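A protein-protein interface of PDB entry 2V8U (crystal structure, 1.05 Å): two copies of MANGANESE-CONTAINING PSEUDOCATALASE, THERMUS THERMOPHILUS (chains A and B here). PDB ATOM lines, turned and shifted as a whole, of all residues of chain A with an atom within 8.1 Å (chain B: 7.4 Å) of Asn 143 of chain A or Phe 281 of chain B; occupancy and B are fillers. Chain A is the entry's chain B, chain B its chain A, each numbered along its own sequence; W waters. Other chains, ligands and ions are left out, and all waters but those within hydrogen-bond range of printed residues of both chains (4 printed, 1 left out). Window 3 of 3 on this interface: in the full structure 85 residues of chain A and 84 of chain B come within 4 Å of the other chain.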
ATOM      1  N   GLN A  46      14.373  10.603  -5.360  1.00  0.00           N
ATOM      2  CA  GLN A  46      14.304  11.711  -6.310  1.00  0.00           C
ATOM      3  C   GLN A  46      12.898  12.321  -6.312  1.00  0.00           C
ATOM      4  O   GLN A  46      12.754  13.547  -6.395  1.00  0.00           O
ATOM      5  CB  GLN A  46      14.637  11.230  -7.712  1.00  0.00           C
ATOM      6  CG  GLN A  46      16.125  10.876  -7.890  1.00  0.00           C
ATOM      7  CD  GLN A  46      16.365  10.114  -9.160  1.00  0.00           C
ATOM      8  OE1 GLN A  46      15.481  10.062 -10.014  1.00  0.00           O
ATOM      9  NE2 GLN A  46      17.534   9.534  -9.308  1.00  0.00           N
ATOM     10  N   ASN A  49      12.527  14.515  -3.292  1.00  0.00           N
ATOM     11  CA  ASN A  49      13.467  15.629  -3.352  1.00  0.00           C
ATOM     12  C   ASN A  49      13.223  16.556  -4.535  1.00  0.00           C
ATOM     13  O   ASN A  49      13.949  17.554  -4.708  1.00  0.00           O
ATOM     14  CB  ASN A  49      14.879  15.064  -3.375  1.00  0.00           C
ATOM     15  CG  ASN A  49      15.269  14.319  -2.113  1.00  0.00           C
ATOM     16  OD1 ASN A  49      14.637  14.480  -1.059  1.00  0.00           O
ATOM     17  ND2 ASN A  49      16.343  13.547  -2.197  1.00  0.00           N
ATOM     18  N   PHE A  50      12.221  16.267  -5.350  1.00  0.00           N
ATOM     19  CA  PHE A  50      12.015  16.948  -6.631  1.00  0.00           C
ATOM     20  C   PHE A  50      11.678  18.402  -6.418  1.00  0.00           C
ATOM     21  O   PHE A  50      10.754  18.739  -5.666  1.00  0.00           O
ATOM     22  CB  PHE A  50      10.893  16.238  -7.379  1.00  0.00           C
ATOM     23  CG  PHE A  50      10.817  16.547  -8.845  1.00  0.00           C
ATOM     24  CD1 PHE A  50      10.290  17.732  -9.304  1.00  0.00           C
ATOM     25  CD2 PHE A  50      11.285  15.639  -9.786  1.00  0.00           C
ATOM     26  CE1 PHE A  50      10.237  18.035 -10.651  1.00  0.00           C
ATOM     27  CE2 PHE A  50      11.197  15.925 -11.153  1.00  0.00           C
ATOM     28  CZ  PHE A  50      10.713  17.122 -11.569  1.00  0.00           C
ATOM     29  N   ARG A  51      12.401  19.302  -7.073  1.00  0.00           N
ATOM     30  CA  ARG A  51      12.128  20.733  -7.075  1.00  0.00           C
ATOM     31  C   ARG A  51      11.446  21.108  -8.379  1.00  0.00           C
ATOM     32  O   ARG A  51      11.871  20.731  -9.460  1.00  0.00           O
ATOM     33  CB  ARG A  51      13.427  21.536  -6.918  1.00  0.00           C
ATOM     34  CG  ARG A  51      14.089  21.306  -5.566  1.00  0.00           C
ATOM     35  CD  ARG A  51      15.526  21.754  -5.623  1.00  0.00           C
ATOM     36  NE  ARG A  51      16.268  21.535  -4.386  1.00  0.00           N
ATOM     37  CZ  ARG A  51      16.407  22.435  -3.435  1.00  0.00           C
ATOM     38  NH1 ARG A  51      15.827  23.622  -3.516  1.00  0.00           N
ATOM     39  NH2 ARG A  51      17.123  22.138  -2.373  1.00  0.00           N
ATOM     40  N   LEU A  56       7.672  21.685 -13.357  1.00  0.00           N
ATOM     41  CA  LEU A  56       8.238  20.612 -14.152  1.00  0.00           C
ATOM     42  C   LEU A  56       7.364  19.357 -13.979  1.00  0.00           C
ATOM     43  O   LEU A  56       7.873  18.226 -13.980  1.00  0.00           O
ATOM     44  CB  LEU A  56       9.691  20.346 -13.768  1.00  0.00           C
ATOM     45  CG  LEU A  56      10.623  21.498 -14.087  1.00  0.00           C
ATOM     46  CD1 LEU A  56      11.960  21.359 -13.336  1.00  0.00           C
ATOM     47  CD2 LEU A  56      10.867  21.632 -15.579  1.00  0.00           C
ATOM     48  N   ILE A  63       8.789  10.382 -12.596  1.00  0.00           N
ATOM     49  CA  ILE A  63       9.649   9.770 -11.572  1.00  0.00           C
ATOM     50  C   ILE A  63       8.793   9.231 -10.420  1.00  0.00           C
ATOM     51  O   ILE A  63       9.053   8.145  -9.914  1.00  0.00           O
ATOM     52  CB  ILE A  63      10.721  10.781 -11.116  1.00  0.00           C
ATOM     53  CG1 ILE A  63      11.707  11.130 -12.265  1.00  0.00           C
ATOM     54  CG2 ILE A  63      11.513  10.217  -9.939  1.00  0.00           C
ATOM     55  CD1 ILE A  63      12.699  12.194 -11.923  1.00  0.00           C
ATOM     56  N   PHE A 139      21.328   7.881  -5.973  1.00  0.00           N
ATOM     57  CA  PHE A 139      21.795   9.133  -6.520  1.00  0.00           C
ATOM     58  C   PHE A 139      20.612  10.088  -6.584  1.00  0.00           C
ATOM     59  O   PHE A 139      19.652   9.846  -7.303  1.00  0.00           O
ATOM     60  CB  PHE A 139      22.360   8.904  -7.931  1.00  0.00           C
ATOM     61  CG  PHE A 139      22.959  10.128  -8.524  1.00  0.00           C
ATOM     62  CD1 PHE A 139      24.260  10.483  -8.231  1.00  0.00           C
ATOM     63  CD2 PHE A 139      22.238  10.967  -9.380  1.00  0.00           C
ATOM     64  CE1 PHE A 139      24.838  11.621  -8.764  1.00  0.00           C
ATOM     65  CE2 PHE A 139      22.804  12.099  -9.918  1.00  0.00           C
ATOM     66  CZ  PHE A 139      24.106  12.415  -9.629  1.00  0.00           C
ATOM     67  N   THR A 140      20.667  11.159  -5.790  1.00  0.00           N
ATOM     68  CA  THR A 140      19.598  12.143  -5.742  1.00  0.00           C
ATOM     69  C   THR A 140      20.241  13.524  -5.632  1.00  0.00           C
ATOM     70  O   THR A 140      20.503  14.059  -4.549  1.00  0.00           O
ATOM     71  CB  THR A 140      18.558  11.792  -4.689  1.00  0.00           C
ATOM     72  OG1 THR A 140      17.534  12.771  -4.652  1.00  0.00           O
ATOM     73  CG2 THR A 140      19.083  11.598  -3.277  1.00  0.00           C
ATOM     74  N   SER A 141      20.556  14.087  -6.802  1.00  0.00           N
ATOM     75  CA  SER A 141      21.352  15.299  -6.882  1.00  0.00           C
ATOM     76  C   SER A 141      20.539  16.579  -6.838  1.00  0.00           C
ATOM     77  O   SER A 141      21.113  17.662  -6.721  1.00  0.00           O
ATOM     78  CB  SER A 141      22.153  15.302  -8.179  1.00  0.00           C
ATOM     79  OG  SER A 141      21.334  15.610  -9.314  1.00  0.00           O
ATOM     80  N   GLY A 142      19.240  16.475  -7.051  1.00  0.00           N
ATOM     81  CA  GLY A 142      18.404  17.651  -7.185  1.00  0.00           C
ATOM     82  C   GLY A 142      18.410  18.285  -8.579  1.00  0.00           C
ATOM     83  O   GLY A 142      17.550  19.137  -8.838  1.00  0.00           O
ATOM     84  N   ASN A 143      19.348  17.932  -9.451  1.00  0.00           N
ATOM     85  CA  ASN A 143      19.433  18.448 -10.815  1.00  0.00           C
ATOM     86  C   ASN A 143      18.715  17.474 -11.736  1.00  0.00           C
ATOM     87  O   ASN A 143      19.070  16.307 -11.803  1.00  0.00           O
ATOM     88  CB  ASN A 143      20.898  18.623 -11.223  1.00  0.00           C
ATOM     89  CG  ASN A 143      21.047  19.187 -12.618  1.00  0.00           C
ATOM     90  OD1 ASN A 143      21.006  18.465 -13.613  1.00  0.00           O
ATOM     91  ND2 ASN A 143      21.230  20.520 -12.701  1.00  0.00           N
ATOM     92  N   LEU A 144      17.648  17.966 -12.385  1.00  0.00           N
ATOM     93  CA  LEU A 144      16.754  17.075 -13.113  1.00  0.00           C
ATOM     94  C   LEU A 144      17.494  16.304 -14.212  1.00  0.00           C
ATOM     95  O   LEU A 144      17.325  15.080 -14.325  1.00  0.00           O
ATOM     96  CB  LEU A 144      15.583  17.883 -13.696  1.00  0.00           C
ATOM     97  CG  LEU A 144      14.600  17.061 -14.518  1.00  0.00           C
ATOM     98  CD1 LEU A 144      14.014  15.871 -13.741  1.00  0.00           C
ATOM     99  CD2 LEU A 144      13.487  17.953 -15.060  1.00  0.00           C
ATOM    100  N   ILE A 145      18.237  16.986 -15.066  1.00  0.00           N
ATOM    101  CA  ILE A 145      18.875  16.304 -16.191  1.00  0.00           C
ATOM    102  C   ILE A 145      19.927  15.319 -15.693  1.00  0.00           C
ATOM    103  O   ILE A 145      20.027  14.207 -16.226  1.00  0.00           O
ATOM    104  CB  ILE A 145      19.438  17.336 -17.201  1.00  0.00           C
ATOM    105  CG1 ILE A 145      18.263  18.044 -17.896  1.00  0.00           C
ATOM    106  CG2 ILE A 145      20.378  16.657 -18.212  1.00  0.00           C
ATOM    107  CD1 ILE A 145      18.671  19.285 -18.652  1.00  0.00           C
ATOM    108  N   LEU A 146      20.725  15.705 -14.702  1.00  0.00           N
ATOM    109  CA  LEU A 146      21.745  14.796 -14.158  1.00  0.00           C
ATOM    110  C   LEU A 146      21.079  13.535 -13.609  1.00  0.00           C
ATOM    111  O   LEU A 146      21.567  12.419 -13.832  1.00  0.00           O
ATOM    112  CB  LEU A 146      22.565  15.533 -13.122  1.00  0.00           C
ATOM    113  CG  LEU A 146      23.744  14.776 -12.514  1.00  0.00           C
ATOM    114  CD1 LEU A 146      24.784  14.390 -13.551  1.00  0.00           C
ATOM    115  CD2 LEU A 146      24.365  15.666 -11.420  1.00  0.00           C
ATOM    116  N   ASP A 147      19.996  13.688 -12.844  1.00  0.00           N
ATOM    117  CA  ASP A 147      19.272  12.548 -12.322  1.00  0.00           C
ATOM    118  C   ASP A 147      18.709  11.665 -13.437  1.00  0.00           C
ATOM    119  O   ASP A 147      18.754  10.446 -13.341  1.00  0.00           O
ATOM    120  CB  ASP A 147      18.153  12.986 -11.385  1.00  0.00           C
ATOM    121  CG  ASP A 147      18.563  13.466 -10.013  1.00  0.00           C
ATOM    122  OD1 ASP A 147      19.761  13.363  -9.625  1.00  0.00           O
ATOM    123  OD2 ASP A 147      17.627  13.924  -9.320  1.00  0.00           O
ATOM    124  N   LEU A 148      18.135  12.284 -14.471  1.00  0.00           N
ATOM    125  CA  LEU A 148      17.561  11.501 -15.533  1.00  0.00           C
ATOM    126  C   LEU A 148      18.609  10.733 -16.334  1.00  0.00           C
ATOM    127  O   LEU A 148      18.377   9.597 -16.740  1.00  0.00           O
ATOM    128  CB  LEU A 148      16.750  12.388 -16.481  1.00  0.00           C
ATOM    129  CG  LEU A 148      15.398  12.857 -15.930  1.00  0.00           C
ATOM    130  CD1 LEU A 148      14.859  13.961 -16.855  1.00  0.00           C
ATOM    131  CD2 LEU A 148      14.397  11.725 -15.825  1.00  0.00           C
ATOM    132  N   LEU A 149      19.784  11.349 -16.547  1.00  0.00           N
ATOM    133  CA  LEU A 149      20.899  10.659 -17.191  1.00  0.00           C
ATOM    134  C   LEU A 149      21.322   9.462 -16.331  1.00  0.00           C
ATOM    135  O   LEU A 149      21.508   8.355 -16.836  1.00  0.00           O
ATOM    136  CB  LEU A 149      22.038  11.670 -17.399  1.00  0.00           C
ATOM    137  CG  LEU A 149      23.333  11.068 -17.960  1.00  0.00           C
ATOM    138  CD1 LEU A 149      23.127  10.453 -19.345  1.00  0.00           C
ATOM    139  CD2 LEU A 149      24.399  12.130 -17.977  1.00  0.00           C
ATOM    140  N   HIS A 150      21.465   9.702 -15.028  1.00  0.00           N
ATOM    141  CA  HIS A 150      21.736   8.603 -14.080  1.00  0.00           C
ATOM    142  C   HIS A 150      20.720   7.492 -14.261  1.00  0.00           C
ATOM    143  O   HIS A 150      21.085   6.310 -14.316  1.00  0.00           O
ATOM    144  CB  HIS A 150      21.680   9.116 -12.650  1.00  0.00           C
ATOM    145  CG  HIS A 150      21.709   8.015 -11.655  1.00  0.00           C
ATOM    146  ND1 HIS A 150      20.549   7.407 -11.225  1.00  0.00           N
ATOM    147  CD2 HIS A 150      22.724   7.307 -11.096  1.00  0.00           C
ATOM    148  CE1 HIS A 150      20.895   6.409 -10.396  1.00  0.00           C
ATOM    149  NE2 HIS A 150      22.200   6.308 -10.291  1.00  0.00           N
ATOM    150  N   VAL B  97      22.449  34.460  -8.468  1.00  0.00           N
ATOM    151  CA  VAL B  97      23.414  33.702  -7.680  1.00  0.00           C
ATOM    152  C   VAL B  97      24.685  33.500  -8.482  1.00  0.00           C
ATOM    153  O   VAL B  97      24.635  33.062  -9.623  1.00  0.00           O
ATOM    154  CB  VAL B  97      22.810  32.367  -7.233  1.00  0.00           C
ATOM    155  CG1 VAL B  97      23.849  31.508  -6.542  1.00  0.00           C
ATOM    156  CG2 VAL B  97      21.594  32.620  -6.304  1.00  0.00           C
ATOM    157  N   PRO B  99      28.341  31.582  -8.434  1.00  0.00           N
ATOM    158  CA  PRO B  99      29.184  30.569  -7.766  1.00  0.00           C
ATOM    159  C   PRO B  99      30.495  31.137  -7.262  1.00  0.00           C
ATOM    160  O   PRO B  99      31.015  30.643  -6.211  1.00  0.00           O
ATOM    161  CB  PRO B  99      29.418  29.509  -8.823  1.00  0.00           C
ATOM    162  CG  PRO B  99      28.210  29.589  -9.566  1.00  0.00           C
ATOM    163  CD  PRO B  99      27.821  31.066  -9.707  1.00  0.00           C
ATOM    164  N   LEU B 104      27.697  28.755  -0.940  1.00  0.00           N
ATOM    165  CA  LEU B 104      27.561  27.612  -0.046  1.00  0.00           C
ATOM    166  C   LEU B 104      28.578  27.681   1.089  1.00  0.00           C
ATOM    167  O   LEU B 104      28.832  26.665   1.747  1.00  0.00           O
ATOM    168  CB  LEU B 104      27.622  26.291  -0.789  1.00  0.00           C
ATOM    169  CG  LEU B 104      26.539  26.066  -1.838  1.00  0.00           C
ATOM    170  CD1 LEU B 104      26.751  24.718  -2.498  1.00  0.00           C
ATOM    171  CD2 LEU B 104      25.130  26.180  -1.284  1.00  0.00           C
ATOM    172  N   GLY B 119      23.798  15.579  -2.221  1.00  0.00           N
ATOM    173  CA  GLY B 119      22.464  16.102  -2.439  1.00  0.00           C
ATOM    174  C   GLY B 119      22.514  17.512  -2.960  1.00  0.00           C
ATOM    175  O   GLY B 119      23.490  18.242  -2.787  1.00  0.00           O
ATOM    176  N   GLY B 120      21.430  17.928  -3.607  1.00  0.00           N
ATOM    177  CA  GLY B 120      21.211  19.317  -3.960  1.00  0.00           C
ATOM    178  C   GLY B 120      20.491  20.026  -2.832  1.00  0.00           C
ATOM    179  O   GLY B 120      19.356  20.490  -3.028  1.00  0.00           O
ATOM    180  N   ASN B 122      19.222  18.374  -0.231  1.00  0.00           N
ATOM    181  CA  ASN B 122      18.072  17.519  -0.091  1.00  0.00           C
ATOM    182  C   ASN B 122      18.421  16.288   0.737  1.00  0.00           C
ATOM    183  O   ASN B 122      19.579  15.987   1.003  1.00  0.00           O
ATOM    184  CB  ASN B 122      17.449  17.163  -1.450  1.00  0.00           C
ATOM    185  CG  ASN B 122      18.379  16.510  -2.455  1.00  0.00           C
ATOM    186  OD1 ASN B 122      18.982  15.386  -2.145  1.00  0.00           O
ATOM    187  ND2 ASN B 122      18.560  17.070  -3.583  1.00  0.00           N
ATOM    188  N   HIS B 276      13.640  26.610  -6.076  1.00  0.00           N
ATOM    189  CA  HIS B 276      14.918  26.720  -6.742  1.00  0.00           C
ATOM    190  C   HIS B 276      16.042  27.051  -5.768  1.00  0.00           C
ATOM    191  O   HIS B 276      15.902  27.921  -4.932  1.00  0.00           O
ATOM    192  CB  HIS B 276      14.795  27.810  -7.831  1.00  0.00           C
ATOM    193  CG  HIS B 276      16.018  28.028  -8.660  1.00  0.00           C
ATOM    194  ND1 HIS B 276      16.324  29.279  -9.142  1.00  0.00           N
ATOM    195  CD2 HIS B 276      16.966  27.170  -9.076  1.00  0.00           C
ATOM    196  CE1 HIS B 276      17.427  29.153  -9.847  1.00  0.00           C
ATOM    197  NE2 HIS B 276      17.862  27.892  -9.819  1.00  0.00           N
ATOM    198  N   ASP B 277      17.158  26.331  -5.868  1.00  0.00           N
ATOM    199  CA  ASP B 277      18.404  26.657  -5.180  1.00  0.00           C
ATOM    200  C   ASP B 277      19.476  26.670  -6.252  1.00  0.00           C
ATOM    201  O   ASP B 277      19.993  25.626  -6.647  1.00  0.00           O
ATOM    202  CB  ASP B 277      18.680  25.666  -4.048  1.00  0.00           C
ATOM    203  CG  ASP B 277      19.875  25.993  -3.199  1.00  0.00           C
ATOM    204  OD1 ASP B 277      20.804  26.682  -3.726  1.00  0.00           O
ATOM    205  OD2 ASP B 277      19.921  25.523  -2.031  1.00  0.00           O
ATOM    206  N   ALA B 278      19.768  27.859  -6.773  1.00  0.00           N
ATOM    207  CA  ALA B 278      20.692  27.984  -7.901  1.00  0.00           C
ATOM    208  C   ALA B 278      22.102  27.490  -7.570  1.00  0.00           C
ATOM    209  O   ALA B 278      22.732  26.873  -8.417  1.00  0.00           O
ATOM    210  CB  ALA B 278      20.759  29.422  -8.381  1.00  0.00           C
ATOM    211  N   ALA B 279      22.570  27.777  -6.352  1.00  0.00           N
ATOM    212  CA  ALA B 279      23.919  27.316  -5.969  1.00  0.00           C
ATOM    213  C   ALA B 279      24.001  25.788  -5.944  1.00  0.00           C
ATOM    214  O   ALA B 279      25.076  25.206  -6.113  1.00  0.00           O
ATOM    215  CB  ALA B 279      24.275  27.854  -4.623  1.00  0.00           C
ATOM    216  N   GLU B 280      22.890  25.102  -5.746  1.00  0.00           N
ATOM    217  CA  GLU B 280      22.841  23.653  -5.813  1.00  0.00           C
ATOM    218  C   GLU B 280      22.524  23.147  -7.212  1.00  0.00           C
ATOM    219  O   GLU B 280      22.462  21.938  -7.428  1.00  0.00           O
ATOM    220  CB  GLU B 280      21.845  23.073  -4.789  1.00  0.00           C
ATOM    221  CG  GLU B 280      22.121  23.422  -3.319  1.00  0.00           C
ATOM    222  CD  GLU B 280      23.297  22.693  -2.680  1.00  0.00           C
ATOM    223  OE1 GLU B 280      23.869  21.765  -3.360  1.00  0.00           O
ATOM    224  OE2 GLU B 280      23.657  23.027  -1.543  1.00  0.00           O
ATOM    225  N   PHE B 281      22.272  24.052  -8.151  1.00  0.00           N
ATOM    226  CA  PHE B 281      21.945  23.672  -9.507  1.00  0.00           C
ATOM    227  C   PHE B 281      20.652  22.830  -9.552  1.00  0.00           C
ATOM    228  O   PHE B 281      20.503  21.925 -10.364  1.00  0.00           O
ATOM    229  CB  PHE B 281      23.104  22.980 -10.241  1.00  0.00           C
ATOM    230  CG  PHE B 281      24.416  23.642  -9.969  1.00  0.00           C
ATOM    231  CD1 PHE B 281      24.673  24.916 -10.420  1.00  0.00           C
ATOM    232  CD2 PHE B 281      25.373  23.037  -9.189  1.00  0.00           C
ATOM    233  CE1 PHE B 281      25.844  25.568 -10.110  1.00  0.00           C
ATOM    234  CE2 PHE B 281      26.530  23.700  -8.833  1.00  0.00           C
ATOM    235  CZ  PHE B 281      26.773  24.972  -9.315  1.00  0.00           C
ATOM    236  N   ALA B 282      19.700  23.193  -8.662  1.00  0.00           N
ATOM    237  CA  ALA B 282      18.568  22.313  -8.371  1.00  0.00           C
ATOM    238  C   ALA B 282      17.281  23.141  -8.499  1.00  0.00           C
ATOM    239  O   ALA B 282      17.091  24.088  -7.736  1.00  0.00           O
ATOM    240  CB  ALA B 282      18.731  21.707  -7.003  1.00  0.00           C
ATOM    241  N   PRO B 283      16.370  22.834  -9.438  1.00  0.00           N
ATOM    242  CA  PRO B 283      16.430  21.707 -10.381  1.00  0.00           C
ATOM    243  C   PRO B 283      17.338  21.919 -11.582  1.00  0.00           C
ATOM    244  O   PRO B 283      17.603  20.992 -12.334  1.00  0.00           O
ATOM    245  CB  PRO B 283      14.964  21.551 -10.820  1.00  0.00           C
ATOM    246  CG  PRO B 283      14.424  22.962 -10.762  1.00  0.00           C
ATOM    247  CD  PRO B 283      15.113  23.610  -9.586  1.00  0.00           C
ATOM    248  N   GLU B 284      17.796  23.168 -11.767  1.00  0.00           N
ATOM    249  CA  GLU B 284      18.788  23.545 -12.748  1.00  0.00           C
ATOM    250  C   GLU B 284      19.457  24.806 -12.232  1.00  0.00           C
ATOM    251  O   GLU B 284      18.910  25.484 -11.353  1.00  0.00           O
ATOM    252  CB  GLU B 284      18.109  23.784 -14.128  1.00  0.00           C
ATOM    253  CG  GLU B 284      19.069  24.016 -15.302  1.00  0.00           C
ATOM    254  CD  GLU B 284      20.128  22.920 -15.398  1.00  0.00           C
ATOM    255  OE1 GLU B 284      19.909  21.955 -16.178  1.00  0.00           O
ATOM    256  OE2 GLU B 284      21.170  23.064 -14.695  1.00  0.00           O
ATOM    257  N   PHE B 285      20.634  25.168 -12.760  1.00  0.00           N
ATOM    258  CA  PHE B 285      21.244  26.431 -12.376  1.00  0.00           C
ATOM    259  C   PHE B 285      20.262  27.603 -12.537  1.00  0.00           C
ATOM    260  O   PHE B 285      20.034  28.358 -11.600  1.00  0.00           O
ATOM    261  CB  PHE B 285      22.542  26.675 -13.161  1.00  0.00           C
ATOM    262  CG  PHE B 285      23.242  27.947 -12.781  1.00  0.00           C
ATOM    263  CD1 PHE B 285      23.503  28.309 -11.476  1.00  0.00           C
ATOM    264  CD2 PHE B 285      23.622  28.827 -13.782  1.00  0.00           C
ATOM    265  CE1 PHE B 285      24.150  29.501 -11.157  1.00  0.00           C
ATOM    266  CE2 PHE B 285      24.295  30.022 -13.437  1.00  0.00           C
ATOM    267  CZ  PHE B 285      24.495  30.349 -12.136  1.00  0.00           C
ATOM    268  N   HIS B 286      19.699  27.727 -13.742  1.00  0.00           N
ATOM    269  CA  HIS B 286      18.625  28.677 -14.011  1.00  0.00           C
ATOM    270  C   HIS B 286      17.553  27.876 -14.752  1.00  0.00           C
ATOM    271  O   HIS B 286      17.776  27.513 -15.900  1.00  0.00           O
ATOM    272  CB  HIS B 286      19.092  29.826 -14.861  1.00  0.00           C
ATOM    273  CG  HIS B 286      18.061  30.881 -15.056  1.00  0.00           C
ATOM    274  ND1 HIS B 286      16.856  30.660 -15.696  1.00  0.00           N
ATOM    275  CD2 HIS B 286      18.064  32.156 -14.631  1.00  0.00           C
ATOM    276  CE1 HIS B 286      16.189  31.812 -15.697  1.00  0.00           C
ATOM    277  NE2 HIS B 286      16.898  32.737 -15.065  1.00  0.00           N
ATOM    278  N   PRO B 287      16.429  27.522 -14.102  1.00  0.00           N
ATOM    279  CA  PRO B 287      15.445  26.601 -14.688  1.00  0.00           C
ATOM    280  C   PRO B 287      14.459  27.240 -15.640  1.00  0.00           C
ATOM    281  O   PRO B 287      13.530  26.564 -16.050  1.00  0.00           O
ATOM    282  CB  PRO B 287      14.758  26.016 -13.458  1.00  0.00           C
ATOM    283  CG  PRO B 287      14.802  27.132 -12.466  1.00  0.00           C
ATOM    284  CD  PRO B 287      16.174  27.729 -12.671  1.00  0.00           C
ATOM    285  N   LEU B 290      13.878  25.226 -18.861  1.00  0.00           N
ATOM    286  CA  LEU B 290      13.218  23.941 -18.635  1.00  0.00           C
ATOM    287  C   LEU B 290      11.724  24.164 -18.304  1.00  0.00           C
ATOM    288  O   LEU B 290      10.881  23.402 -18.759  1.00  0.00           O
ATOM    289  CB  LEU B 290      13.873  23.146 -17.515  1.00  0.00           C
ATOM    290  CG  LEU B 290      15.365  22.783 -17.750  1.00  0.00           C
ATOM    291  CD1 LEU B 290      15.800  21.754 -16.765  1.00  0.00           C
ATOM    292  CD2 LEU B 290      15.678  22.327 -19.172  1.00  0.00           C
HETATM  293  O   HOH W   1      21.767  19.953 -15.937  1.00  0.00           O
HETATM  294  O   HOH W   2      15.219  26.481  -2.515  1.00  0.00           O
HETATM  295  O   HOH W   3      16.500  18.726  -4.396  1.00  0.00           O
HETATM  296  O   HOH W   4      17.789  24.516  -0.824  1.00  0.00           O
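CB of Asp 277 of chain B touches NH1 of Arg 51 of chain A (3.5 Å).
Arg 51 of chain A touches Pro 283 of chain B.
CD1 of Leu 56 of chain A touches CG of Pro 283 of chain B, at 3.9 Å.
Thr 140 of chain A touches Gly 119 of chain B (O to CA, 3.5 Å).
Ser 141 of chain A touches Asn 122 of chain B.
Asn 122 of chain B touches Gly 142 of chain A.
CA of Ala 282 of chain B touches O of Gly 142 of chain A (3.4 Å).
Gly 142 of chain A touches Pro 283 of chain B (O to CA, 3.2 Å).
Asn 143 of chain A touches Pro 283 of chain B.
Ile 145 of chain A touches Glu 284 of chain B (CD1 to OE1, 3.8 Å).
Water W4 lies within hydrogen-bond range of the side-chain carboxylate (OD2) of Asp 277 of chain B (2.6 Å) and the guanidinium group (NH2) of Arg 51 of chain A (2.9 Å).
Water W1 lies within hydrogen-bond range of OE1 of Glu 284 of chain B (2.7 Å) and OD1 of Asn 143 of chain A (2.9 Å).
Water W2 lies within hydrogen-bond range of the backbone carbonyl oxygen (O) of His 276 of chain B (2.9 Å) and the guanidinium group (NH1) of Arg 51 of chain A (3.1 Å).
O of Gly 120 of chain B sits at hydrogen-bond distance from NH2 of Arg 51 of chain A (2.9 Å).
The backbone carbonyl oxygen (O) of Ser 141 of chain A sits at hydrogen-bond distance from the backbone NH (N) of Gly 120 of chain B.
OD1 of Asn 122 of chain B lies within hydrogen-bond range of ND2 of Asn 49 of chain A (3.2 Å).
O of Thr 140 of chain A sits close to OD1 of Asn 122 of chain B, at 3.1 Å.
The side-chain amide nitrogen (ND2) of Asn 143 of chain A sits at hydrogen-bond distance from the backbone carbonyl oxygen (O) of Phe 281 of chain B, 2.8 Å away.
O of Pro 283 of chain B sits at hydrogen-bond distance from N of Leu 144 of chain A (3.0 Å).
The side-chain carboxylate of Glu 284 of chain B is in hydrogen-bond range of the side-chain amide nitrogen of Asn 143 of chain A (3.2 Å).
Gly 142 of chain A touches just these residues of chain B: Asn 122 (3.6 Å), Ala 282 (3.4 Å) and Pro 283 (3.2 Å).
Of the printed residues of chain B, Asn 143 of chain A touches Phe 281 (2.8 Å), Pro 283 (3.5 Å) and Glu 284 (3.2 Å).
His 150 of chain A touches none of the printed residues of chain B.
Pro 99 of chain B touches none of the printed residues of chain A.
Of the printed residues of chain A, Asn 122 of chain B touches Asn 49 (3.2 Å), Thr 140 (3.1 Å), Ser 141 (3.8 Å) and Gly 142 (3.6 Å).
Of chain A, only Asn 143 (2.8 Å) comes within 4 Å of Phe 281 of chain B.
Of the printed residues of chain A, Glu 284 of chain B touches Asn 143 (3.2 Å) and Ile 145 (3.8 Å).
The nearest printed residue of chain A that does not touch Pro 283 of chain B is Ile 145 of chain A (4.9 Å).
No position is printed for both chains.
Of the 19 pairs that touch across the chains among the printed residues, none has its exchanged pair printed and touching as well.
Of the 19 printed residues of chain B, 9 touch a printed residue of chain A.
Printed residues of chain B that touch a printed residue of chain A: Gly 119, Gly 120, Asn 122, Asp 277, Phe 281, Ala 282, Pro 283, Glu 284 and Leu 290.
Hydrophobic or aromatic side chains of chain B that line the printed part of chain A: Phe 281, Ala 282, Pro 283 and Leu 290.
Among the printed residues, 19 pairs touch across the chains.
The backbone NH (N) of Gly 120 of chain B lies close to the side-chain amide nitrogen (ND2) of Asn 122 of chain B.
O of Glu 284 of chain B sits at hydrogen-bond distance from NE2 of His 276 of chain B, 3.0 Å away.
The backbone NH (N) of Ala 279 of chain B lies close to the side-chain carboxylate (OD1) of Asp 277 of chain B.
The backbone NH of Asp 277 of chain B is in hydrogen-bond range of the backbone carbonyl oxygen of Ala 282 of chain B (2.9 Å).
OD1 of Asn 143 of chain A sits close to N of Ile 145 of chain A (3.5 Å).
N of Leu 146 of chain A is in hydrogen-bond range of OD1 of Asn 143 of chain A (3.0 Å).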
